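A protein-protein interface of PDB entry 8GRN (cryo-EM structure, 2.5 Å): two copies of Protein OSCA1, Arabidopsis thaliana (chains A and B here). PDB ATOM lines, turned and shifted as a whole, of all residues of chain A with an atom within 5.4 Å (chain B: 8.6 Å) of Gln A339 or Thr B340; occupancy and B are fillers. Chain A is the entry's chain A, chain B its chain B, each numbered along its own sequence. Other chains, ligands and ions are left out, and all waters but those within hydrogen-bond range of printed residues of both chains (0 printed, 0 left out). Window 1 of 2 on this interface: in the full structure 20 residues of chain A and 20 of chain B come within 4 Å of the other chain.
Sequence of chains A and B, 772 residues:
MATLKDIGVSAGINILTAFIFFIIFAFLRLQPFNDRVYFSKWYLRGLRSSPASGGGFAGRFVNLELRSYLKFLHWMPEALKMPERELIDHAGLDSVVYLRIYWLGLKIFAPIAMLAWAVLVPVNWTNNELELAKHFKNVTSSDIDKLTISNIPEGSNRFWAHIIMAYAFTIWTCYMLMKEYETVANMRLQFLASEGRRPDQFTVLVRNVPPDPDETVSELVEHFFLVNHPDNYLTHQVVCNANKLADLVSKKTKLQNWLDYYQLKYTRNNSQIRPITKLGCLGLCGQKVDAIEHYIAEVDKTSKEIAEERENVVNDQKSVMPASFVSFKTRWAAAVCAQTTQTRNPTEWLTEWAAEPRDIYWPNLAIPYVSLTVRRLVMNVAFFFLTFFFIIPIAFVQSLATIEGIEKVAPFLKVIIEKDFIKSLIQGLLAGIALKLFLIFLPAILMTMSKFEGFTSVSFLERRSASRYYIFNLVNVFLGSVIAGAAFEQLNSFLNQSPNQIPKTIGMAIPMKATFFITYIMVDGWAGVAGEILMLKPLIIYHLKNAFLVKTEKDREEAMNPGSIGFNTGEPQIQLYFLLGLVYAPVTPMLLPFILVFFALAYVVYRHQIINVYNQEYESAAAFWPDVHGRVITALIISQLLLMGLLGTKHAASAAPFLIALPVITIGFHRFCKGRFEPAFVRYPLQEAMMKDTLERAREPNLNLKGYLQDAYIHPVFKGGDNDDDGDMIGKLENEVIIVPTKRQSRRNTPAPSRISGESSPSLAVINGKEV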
ATOM      1  N   ALA A 335      16.919  20.156  32.345  1.00  0.00           N
ATOM      2  CA  ALA A 335      17.136  21.221  31.448  1.00  0.00           C
ATOM      3  C   ALA A 335      17.673  20.751  30.202  1.00  0.00           C
ATOM      4  O   ALA A 335      17.758  21.488  29.324  1.00  0.00           O
ATOM      5  CB  ALA A 335      18.112  22.124  32.041  1.00  0.00           C
ATOM      6  N   VAL A 336      17.987  19.506  30.077  1.00  0.00           N
ATOM      7  CA  VAL A 336      18.477  18.884  28.917  1.00  0.00           C
ATOM      8  C   VAL A 336      17.290  18.226  28.285  1.00  0.00           C
ATOM      9  O   VAL A 336      17.282  18.041  27.136  1.00  0.00           O
ATOM     10  CB  VAL A 336      19.532  17.839  29.332  1.00  0.00           C
ATOM     11  CG1 VAL A 336      19.694  16.713  28.344  1.00  0.00           C
ATOM     12  CG2 VAL A 336      20.857  18.470  29.665  1.00  0.00           C
ATOM     13  N   CYS A 337      16.237  17.899  28.995  1.00  0.00           N
ATOM     14  CA  CYS A 337      15.027  17.336  28.452  1.00  0.00           C
ATOM     15  C   CYS A 337      14.105  18.407  28.007  1.00  0.00           C
ATOM     16  O   CYS A 337      13.253  18.159  27.240  1.00  0.00           O
ATOM     17  CB  CYS A 337      14.407  16.443  29.462  1.00  0.00           C
ATOM     18  SG  CYS A 337      12.977  15.522  29.021  1.00  0.00           S
ATOM     19  N   ALA A 338      14.291  19.632  28.408  1.00  0.00           N
ATOM     20  CA  ALA A 338      13.515  20.709  27.963  1.00  0.00           C
ATOM     21  C   ALA A 338      14.074  21.386  26.761  1.00  0.00           C
ATOM     22  O   ALA A 338      13.325  22.009  26.070  1.00  0.00           O
ATOM     23  CB  ALA A 338      13.416  21.658  29.047  1.00  0.00           C
ATOM     24  N   GLN A 339      15.359  21.283  26.461  1.00  0.00           N
ATOM     25  CA  GLN A 339      15.915  21.863  25.312  1.00  0.00           C
ATOM     26  C   GLN A 339      16.495  20.965  24.311  1.00  0.00           C
ATOM     27  O   GLN A 339      17.285  21.409  23.558  1.00  0.00           O
ATOM     28  CB  GLN A 339      16.855  22.942  25.703  1.00  0.00           C
ATOM     29  CG  GLN A 339      18.016  22.720  26.621  1.00  0.00           C
ATOM     30  CD  GLN A 339      18.293  23.970  27.434  1.00  0.00           C
ATOM     31  OE1 GLN A 339      17.394  24.513  28.039  1.00  0.00           O
ATOM     32  NE2 GLN A 339      19.521  24.426  27.444  1.00  0.00           N
ATOM     33  N   THR A 340      16.015  19.748  24.175  1.00  0.00           N
ATOM     34  CA  THR A 340      16.533  18.748  23.304  1.00  0.00           C
ATOM     35  C   THR A 340      15.342  18.061  22.609  1.00  0.00           C
ATOM     36  O   THR A 340      14.291  18.114  23.148  1.00  0.00           O
ATOM     37  CB  THR A 340      17.429  17.867  24.182  1.00  0.00           C
ATOM     38  OG1 THR A 340      18.797  17.975  23.792  1.00  0.00           O
ATOM     39  CG2 THR A 340      17.010  16.455  24.184  1.00  0.00           C
ATOM     40  N   THR A 341      15.473  17.481  21.405  1.00  0.00           N
ATOM     41  CA  THR A 341      14.422  16.771  20.679  1.00  0.00           C
ATOM     42  C   THR A 341      14.511  15.353  20.982  1.00  0.00           C
ATOM     43  O   THR A 341      15.569  14.836  21.057  1.00  0.00           O
ATOM     44  CB  THR A 341      14.447  17.012  19.182  1.00  0.00           C
ATOM     45  OG1 THR A 341      14.279  15.795  18.484  1.00  0.00           O
ATOM     46  CG2 THR A 341      15.726  17.610  18.789  1.00  0.00           C
ATOM     47  N   TRP A 353       8.998  22.963  30.134  1.00  0.00           N
ATOM     48  CA  TRP A 353       9.360  23.011  31.493  1.00  0.00           C
ATOM     49  C   TRP A 353       8.081  23.213  32.062  1.00  0.00           C
ATOM     50  O   TRP A 353       7.278  23.813  31.466  1.00  0.00           O
ATOM     51  CB  TRP A 353      10.062  24.263  31.767  1.00  0.00           C
ATOM     52  CG  TRP A 353      11.539  24.325  31.791  1.00  0.00           C
ATOM     53  CD1 TRP A 353      12.319  25.069  30.977  1.00  0.00           C
ATOM     54  CD2 TRP A 353      12.418  23.713  32.731  1.00  0.00           C
ATOM     55  NE1 TRP A 353      13.629  24.921  31.310  1.00  0.00           N
ATOM     56  CE2 TRP A 353      13.714  24.092  32.390  1.00  0.00           C
ATOM     57  CE3 TRP A 353      12.235  22.857  33.809  1.00  0.00           C
ATOM     58  CZ2 TRP A 353      14.809  23.661  33.087  1.00  0.00           C
ATOM     59  CZ3 TRP A 353      13.317  22.426  34.482  1.00  0.00           C
ATOM     60  CH2 TRP A 353      14.588  22.829  34.133  1.00  0.00           C
ATOM     61  N   ARG A 683      16.345  30.566  27.873  1.00  0.00           N
ATOM     62  CA  ARG A 683      17.161  29.357  27.878  1.00  0.00           C
ATOM     63  C   ARG A 683      17.981  29.259  29.117  1.00  0.00           C
ATOM     64  O   ARG A 683      18.670  30.173  29.372  1.00  0.00           O
ATOM     65  CB  ARG A 683      18.073  29.392  26.706  1.00  0.00           C
ATOM     66  CG  ARG A 683      18.187  28.079  25.989  1.00  0.00           C
ATOM     67  CD  ARG A 683      17.704  28.187  24.567  1.00  0.00           C
ATOM     68  NE  ARG A 683      17.414  26.872  24.013  1.00  0.00           N
ATOM     69  CZ  ARG A 683      18.335  26.027  23.570  1.00  0.00           C
ATOM     70  NH1 ARG A 683      19.609  26.347  23.611  1.00  0.00           N
ATOM     71  NH2 ARG A 683      17.978  24.862  23.071  1.00  0.00           N
ATOM     72  N   TYR A 684      17.887  28.191  29.915  1.00  0.00           N
ATOM     73  CA  TYR A 684      18.625  28.000  31.160  1.00  0.00           C
ATOM     74  C   TYR A 684      19.937  27.391  30.938  1.00  0.00           C
ATOM     75  O   TYR A 684      20.009  26.263  30.572  1.00  0.00           O
ATOM     76  CB  TYR A 684      17.880  27.097  32.103  1.00  0.00           C
ATOM     77  CG  TYR A 684      18.282  27.219  33.557  1.00  0.00           C
ATOM     78  CD1 TYR A 684      18.607  28.435  34.106  1.00  0.00           C
ATOM     79  CD2 TYR A 684      18.340  26.117  34.373  1.00  0.00           C
ATOM     80  CE1 TYR A 684      18.985  28.549  35.420  1.00  0.00           C
ATOM     81  CE2 TYR A 684      18.711  26.225  35.691  1.00  0.00           C
ATOM     82  CZ  TYR A 684      19.030  27.448  36.205  1.00  0.00           C
ATOM     83  OH  TYR A 684      19.395  27.580  37.517  1.00  0.00           O
ATOM     84  N   LEU A 686      23.513  25.519  31.381  1.00  0.00           N
ATOM     85  CA  LEU A 686      23.792  24.258  32.034  1.00  0.00           C
ATOM     86  C   LEU A 686      24.866  24.364  33.023  1.00  0.00           C
ATOM     87  O   LEU A 686      25.060  23.464  33.770  1.00  0.00           O
ATOM     88  CB  LEU A 686      24.120  23.181  30.997  1.00  0.00           C
ATOM     89  CG  LEU A 686      23.192  22.052  30.579  1.00  0.00           C
ATOM     90  CD1 LEU A 686      21.792  22.522  30.293  1.00  0.00           C
ATOM     91  CD2 LEU A 686      23.780  21.400  29.358  1.00  0.00           C
ATOM     92  N   PHE B 225      34.510  20.968  30.977  1.00  0.00           N
ATOM     93  CA  PHE B 225      33.700  19.855  30.616  1.00  0.00           C
ATOM     94  C   PHE B 225      33.783  18.740  31.551  1.00  0.00           C
ATOM     95  O   PHE B 225      33.011  17.875  31.475  1.00  0.00           O
ATOM     96  CB  PHE B 225      33.985  19.414  29.211  1.00  0.00           C
ATOM     97  CG  PHE B 225      33.487  20.333  28.148  1.00  0.00           C
ATOM     98  CD1 PHE B 225      32.230  20.185  27.637  1.00  0.00           C
ATOM     99  CD2 PHE B 225      34.295  21.314  27.629  1.00  0.00           C
ATOM    100  CE1 PHE B 225      31.765  21.021  26.660  1.00  0.00           C
ATOM    101  CE2 PHE B 225      33.838  22.156  26.658  1.00  0.00           C
ATOM    102  CZ  PHE B 225      32.570  22.009  26.171  1.00  0.00           C
ATOM    103  N   ASN B 228      31.056  20.200  34.071  1.00  0.00           N
ATOM    104  CA  ASN B 228      29.748  20.459  33.521  1.00  0.00           C
ATOM    105  C   ASN B 228      29.117  19.399  32.688  1.00  0.00           C
ATOM    106  O   ASN B 228      27.955  19.460  32.516  1.00  0.00           O
ATOM    107  CB  ASN B 228      29.689  21.819  32.845  1.00  0.00           C
ATOM    108  CG  ASN B 228      29.959  22.952  33.777  1.00  0.00           C
ATOM    109  OD1 ASN B 228      30.870  23.719  33.574  1.00  0.00           O
ATOM    110  ND2 ASN B 228      29.160  23.070  34.802  1.00  0.00           N
ATOM    111  N   HIS B 229      29.837  18.425  32.169  1.00  0.00           N
ATOM    112  CA  HIS B 229      29.339  17.292  31.394  1.00  0.00           C
ATOM    113  C   HIS B 229      30.148  16.260  31.993  1.00  0.00           C
ATOM    114  O   HIS B 229      30.960  15.738  31.332  1.00  0.00           O
ATOM    115  CB  HIS B 229      29.701  17.403  29.962  1.00  0.00           C
ATOM    116  CG  HIS B 229      28.871  18.382  29.214  1.00  0.00           C
ATOM    117  ND1 HIS B 229      27.726  18.018  28.554  1.00  0.00           N
ATOM    118  CD2 HIS B 229      29.009  19.710  29.031  1.00  0.00           C
ATOM    119  CE1 HIS B 229      27.187  19.083  27.999  1.00  0.00           C
ATOM    120  NE2 HIS B 229      27.948  20.123  28.274  1.00  0.00           N
ATOM    121  N   ALA B 333      25.476  11.953  24.298  1.00  0.00           N
ATOM    122  CA  ALA B 333      26.072  12.981  25.066  1.00  0.00           C
ATOM    123  C   ALA B 333      26.554  14.055  24.306  1.00  0.00           C
ATOM    124  O   ALA B 333      26.658  15.106  24.819  1.00  0.00           O
ATOM    125  CB  ALA B 333      27.207  12.415  25.697  1.00  0.00           C
ATOM    126  N   ALA B 334      26.875  13.858  23.070  1.00  0.00           N
ATOM    127  CA  ALA B 334      27.397  14.827  22.190  1.00  0.00           C
ATOM    128  C   ALA B 334      26.360  15.564  21.542  1.00  0.00           C
ATOM    129  O   ALA B 334      26.622  16.616  21.067  1.00  0.00           O
ATOM    130  CB  ALA B 334      28.113  14.107  21.163  1.00  0.00           C
ATOM    131  N   ALA B 335      25.158  15.042  21.490  1.00  0.00           N
ATOM    132  CA  ALA B 335      24.030  15.652  20.906  1.00  0.00           C
ATOM    133  C   ALA B 335      23.316  16.449  21.863  1.00  0.00           C
ATOM    134  O   ALA B 335      22.463  17.124  21.492  1.00  0.00           O
ATOM    135  CB  ALA B 335      23.134  14.602  20.442  1.00  0.00           C
ATOM    136  N   VAL B 336      23.686  16.437  23.099  1.00  0.00           N
ATOM    137  CA  VAL B 336      23.124  17.191  24.143  1.00  0.00           C
ATOM    138  C   VAL B 336      24.024  18.375  24.310  1.00  0.00           C
ATOM    139  O   VAL B 336      23.595  19.364  24.748  1.00  0.00           O
ATOM    140  CB  VAL B 336      23.109  16.324  25.418  1.00  0.00           C
ATOM    141  CG1 VAL B 336      23.125  17.122  26.696  1.00  0.00           C
ATOM    142  CG2 VAL B 336      21.985  15.323  25.411  1.00  0.00           C
ATOM    143  N   CYS B 337      25.278  18.334  23.925  1.00  0.00           N
ATOM    144  CA  CYS B 337      26.186  19.450  23.978  1.00  0.00           C
ATOM    145  C   CYS B 337      26.079  20.272  22.750  1.00  0.00           C
ATOM    146  O   CYS B 337      26.463  21.381  22.756  1.00  0.00           O
ATOM    147  CB  CYS B 337      27.565  18.949  24.201  1.00  0.00           C
ATOM    148  SG  CYS B 337      28.866  20.107  24.432  1.00  0.00           S
ATOM    149  N   ALA B 338      25.490  19.788  21.694  1.00  0.00           N
ATOM    150  CA  ALA B 338      25.275  20.533  20.528  1.00  0.00           C
ATOM    151  C   ALA B 338      23.964  21.238  20.509  1.00  0.00           C
ATOM    152  O   ALA B 338      23.854  22.196  19.803  1.00  0.00           O
ATOM    153  CB  ALA B 338      25.351  19.628  19.407  1.00  0.00           C
ATOM    154  N   GLN B 339      22.961  20.825  21.266  1.00  0.00           N
ATOM    155  CA  GLN B 339      21.728  21.490  21.314  1.00  0.00           C
ATOM    156  C   GLN B 339      21.320  22.072  22.595  1.00  0.00           C
ATOM    157  O   GLN B 339      20.173  22.283  22.769  1.00  0.00           O
ATOM    158  CB  GLN B 339      20.671  20.625  20.734  1.00  0.00           C
ATOM    159  CG  GLN B 339      20.381  19.244  21.233  1.00  0.00           C
ATOM    160  CD  GLN B 339      19.905  18.361  20.096  1.00  0.00           C
ATOM    161  OE1 GLN B 339      20.544  18.296  19.068  1.00  0.00           O
ATOM    162  NE2 GLN B 339      18.793  17.692  20.274  1.00  0.00           N
ATOM    163  N   THR B 340      22.237  22.484  23.442  1.00  0.00           N
ATOM    164  CA  THR B 340      21.987  22.991  24.748  1.00  0.00           C
ATOM    165  C   THR B 340      22.877  24.232  24.954  1.00  0.00           C
ATOM    166  O   THR B 340      23.850  24.322  24.289  1.00  0.00           O
ATOM    167  CB  THR B 340      22.214  21.808  25.696  1.00  0.00           C
ATOM    168  OG1 THR B 340      20.998  21.419  26.334  1.00  0.00           O
ATOM    169  CG2 THR B 340      23.254  22.078  26.703  1.00  0.00           C
ATOM    170  N   THR B 341      22.530  25.210  25.806  1.00  0.00           N
ATOM    171  CA  THR B 341      23.317  26.405  26.104  1.00  0.00           C
ATOM    172  C   THR B 341      24.136  26.153  27.277  1.00  0.00           C
ATOM    173  O   THR B 341      23.685  25.554  28.188  1.00  0.00           O
ATOM    174  CB  THR B 341      22.479  27.657  26.281  1.00  0.00           C
ATOM    175  OG1 THR B 341      22.914  28.383  27.412  1.00  0.00           O
ATOM    176  CG2 THR B 341      21.070  27.299  26.462  1.00  0.00           C
ATOM    177  N   GLN B 342      25.359  26.613  27.288  1.00  0.00           N
ATOM    178  CA  GLN B 342      26.256  26.251  28.301  1.00  0.00           C
ATOM    179  C   GLN B 342      26.605  27.233  29.316  1.00  0.00           C
ATOM    180  O   GLN B 342      26.964  26.853  30.378  1.00  0.00           O
ATOM    181  CB  GLN B 342      27.512  25.738  27.633  1.00  0.00           C
ATOM    182  CG  GLN B 342      27.339  24.897  26.399  1.00  0.00           C
ATOM    183  CD  GLN B 342      27.215  23.448  26.733  1.00  0.00           C
ATOM    184  OE1 GLN B 342      27.829  22.978  27.660  1.00  0.00           O
ATOM    185  NE2 GLN B 342      26.407  22.739  25.992  1.00  0.00           N
ATOM    186  N   THR B 343      26.504  28.507  29.028  1.00  0.00           N
ATOM    187  CA  THR B 343      26.894  29.559  29.929  1.00  0.00           C
ATOM    188  C   THR B 343      25.954  30.729  29.812  1.00  0.00           C
ATOM    189  O   THR B 343      25.138  30.727  28.941  1.00  0.00           O
ATOM    190  CB  THR B 343      28.358  29.908  29.711  1.00  0.00           C
ATOM    191  OG1 THR B 343      28.818  30.780  30.730  1.00  0.00           O
ATOM    192  CG2 THR B 343      28.527  30.564  28.395  1.00  0.00           C
ATOM    193  N   TRP B 349      31.769  30.154  24.746  1.00  0.00           N
ATOM    194  CA  TRP B 349      31.547  28.744  24.860  1.00  0.00           C
ATOM    195  C   TRP B 349      30.472  28.275  23.995  1.00  0.00           C
ATOM    196  O   TRP B 349      29.490  27.839  24.506  1.00  0.00           O
ATOM    197  CB  TRP B 349      31.337  28.287  26.291  1.00  0.00           C
ATOM    198  CG  TRP B 349      32.442  28.400  27.262  1.00  0.00           C
ATOM    199  CD1 TRP B 349      32.526  29.282  28.270  1.00  0.00           C
ATOM    200  CD2 TRP B 349      33.580  27.554  27.380  1.00  0.00           C
ATOM    201  NE1 TRP B 349      33.651  29.070  28.996  1.00  0.00           N
ATOM    202  CE2 TRP B 349      34.325  28.014  28.461  1.00  0.00           C
ATOM    203  CE3 TRP B 349      34.046  26.463  26.669  1.00  0.00           C
ATOM    204  CZ2 TRP B 349      35.503  27.432  28.842  1.00  0.00           C
ATOM    205  CZ3 TRP B 349      35.204  25.889  27.054  1.00  0.00           C
ATOM    206  CH2 TRP B 349      35.923  26.370  28.125  1.00  0.00           C
ATOM    207  N   LEU B 350      30.647  28.281  22.693  1.00  0.00           N
ATOM    208  CA  LEU B 350      29.606  27.955  21.761  1.00  0.00           C
ATOM    209  C   LEU B 350      29.712  26.732  20.958  1.00  0.00           C
ATOM    210  O   LEU B 350      30.230  26.777  19.910  1.00  0.00           O
ATOM    211  CB  LEU B 350      29.376  29.093  20.814  1.00  0.00           C
ATOM    212  CG  LEU B 350      29.219  30.551  21.166  1.00  0.00           C
ATOM    213  CD1 LEU B 350      29.863  31.347  20.058  1.00  0.00           C
ATOM    214  CD2 LEU B 350      27.748  30.867  21.218  1.00  0.00           C
ATOM    215  N   THR B 351      29.110  25.645  21.369  1.00  0.00           N
ATOM    216  CA  THR B 351      29.167  24.343  20.749  1.00  0.00           C
ATOM    217  C   THR B 351      28.257  24.019  19.561  1.00  0.00           C
ATOM    218  O   THR B 351      27.155  24.456  19.539  1.00  0.00           O
ATOM    219  CB  THR B 351      28.890  23.414  21.906  1.00  0.00           C
ATOM    220  OG1 THR B 351      27.617  23.739  22.443  1.00  0.00           O
ATOM    221  CG2 THR B 351      29.884  23.604  22.991  1.00  0.00           C
ATOM    222  N   GLU B 352      28.710  23.283  18.557  1.00  0.00           N
ATOM    223  CA  GLU B 352      27.959  22.942  17.371  1.00  0.00           C
ATOM    224  C   GLU B 352      28.408  21.562  17.143  1.00  0.00           C
ATOM    225  O   GLU B 352      28.826  20.995  18.067  1.00  0.00           O
ATOM    226  CB  GLU B 352      28.377  23.783  16.239  1.00  0.00           C
ATOM    227  CG  GLU B 352      29.861  23.914  16.070  1.00  0.00           C
ATOM    228  CD  GLU B 352      30.252  25.275  15.565  1.00  0.00           C
ATOM    229  OE1 GLU B 352      30.244  25.461  14.333  1.00  0.00           O
ATOM    230  OE2 GLU B 352      30.567  26.149  16.401  1.00  0.00           O
ATOM    231  N   ARG B 683      18.048  18.762  13.472  1.00  0.00           N
ATOM    232  CA  ARG B 683      18.099  18.375  14.877  1.00  0.00           C
ATOM    233  C   ARG B 683      18.138  16.895  15.034  1.00  0.00           C
ATOM    234  O   ARG B 683      17.284  16.283  14.511  1.00  0.00           O
ATOM    235  CB  ARG B 683      16.886  18.894  15.559  1.00  0.00           C
ATOM    236  CG  ARG B 683      17.160  19.493  16.908  1.00  0.00           C
ATOM    237  CD  ARG B 683      16.791  20.952  16.945  1.00  0.00           C
ATOM    238  NE  ARG B 683      17.430  21.625  18.066  1.00  0.00           N
ATOM    239  CZ  ARG B 683      17.010  21.550  19.322  1.00  0.00           C
ATOM    240  NH1 ARG B 683      15.950  20.837  19.628  1.00  0.00           N
ATOM    241  NH2 ARG B 683      17.644  22.206  20.271  1.00  0.00           N
ATOM    242  N   LEU B 686      17.188  12.210  20.217  1.00  0.00           N
ATOM    243  CA  LEU B 686      17.951  11.555  21.257  1.00  0.00           C
ATOM    244  C   LEU B 686      17.586  10.147  21.419  1.00  0.00           C
ATOM    245  O   LEU B 686      18.264   9.443  22.090  1.00  0.00           O
ATOM    246  CB  LEU B 686      17.801  12.306  22.582  1.00  0.00           C
ATOM    247  CG  LEU B 686      18.862  13.189  23.218  1.00  0.00           C
ATOM    248  CD1 LEU B 686      19.485  14.148  22.240  1.00  0.00           C
ATOM    249  CD2 LEU B 686      18.218  13.945  24.347  1.00  0.00           C
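O of Ala A335 lies close to OE1 of Gln A339.
The backbone carbonyl oxygen of Ala B335 sits close to the side-chain amide oxygen of Gln B339, 3.3 Å away.
The side-chain amide oxygen (OE1) of Gln B342 is in hydrogen-bond range of a ring nitrogen (NE2) of His B229, 2.9 Å away.
The side-chain amide nitrogen (NE2) of Gln B342 lies close to the backbone carbonyl oxygen (O) of Thr B340 (3.5 Å).
Among the printed residues, merely in contact across the chains: Val A336 with Val B336 (3.8 Å), Gln A339 with Thr B340 (3.3 Å), Gln A339 with Thr B341 (3.4 Å), Thr A340 with Gln B339 (3.3 Å), Thr A340 with Leu B686 (2.8 Å), Thr A341 with Gln B339 (3.4 Å), Thr A341 with Arg B683 (3.0 Å), Arg A683 with Thr B341 (3.0 Å), Arg A683 with Arg B683 (3.9 Å), Leu A686 with Thr B340 (2.8 Å) and Leu A686 with Gln B342 (3.8 Å).
No residue of chain B comes within 4 Å of Ala A338.
Gln A339 touches four residues of chain B.
Thr A340 touches two residues of chain B.
Phe B225 touches none of the printed residues of chain A.
Of the printed residues of chain A, Val B336 touches Val A336.
Thr B340 touches just these residues of chain A: Gln A339 (3.3 Å) and Leu A686 (2.8 Å).
Printed residues of chain A within 4 Å of Thr B341: Gln A339, Arg A683 and Leu A686.
Of the printed residues of chain A, Gln B342 touches Leu A686.
Printed residues of chain A within 4 Å of Arg B683: Gln A339, Thr A341 and Arg A683.
The nearest residue of chain A that does not touch Thr B340 is Arg A683 (4.1 Å).
The nearest printed residue of chain B that does not touch Leu A686 is Asn B228 (4.2 Å).
Hydrophobic or aromatic side chains of chain A within 4 Å of the printed part of chain B: Val A336 and Leu A686.
Of the 20 printed residues of chain B, 7 touch a printed residue of chain A.
Hydrophobic or aromatic side chains of chain B that line the printed part of chain A: Val B336 and Leu B686.
Among the printed residues, 16 pairs touch across the chains.
Among the printed residues, no Asp or Glu carboxylate lies within 4 Å of a Lys or Arg side-chain nitrogen of the other chain.
The backbone carbonyl oxygen (O) of Thr B341 is in hydrogen-bond range of the backbone NH (N) of Leu A686, 3.2 Å away.
The backbone carbonyl oxygen (O) of Gln B339 is in hydrogen-bond range of the guanidinium group (NH2) of Arg A683.
O of Gln A339 lies close to O of Gln B339 (3.1 Å).
O of Gln A339 sits at hydrogen-bond distance from NH2 of Arg B683 (3.4 Å).
O of Thr A341 lies within hydrogen-bond range of N of Leu B686 (3.2 Å).
Gln B339 touches its own counterpart, Gln A339.
Gln A339 touches Thr B340, and with the chains exchanged Thr A340 touches Gln B339.
Gln A339 touches Arg B683, and with the chains exchanged Arg A683 touches Gln B339.
Thr A341 touches Leu B686, and with the chains exchanged Leu A686 touches Thr B341.
Positions printed for both chains: 335, 336, 337, 338, 339, 340, 341, 683 and 686.
Of the 16 pairs that touch across the chains among the printed residues, 15 have their exchanged pair printed and touching as well.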
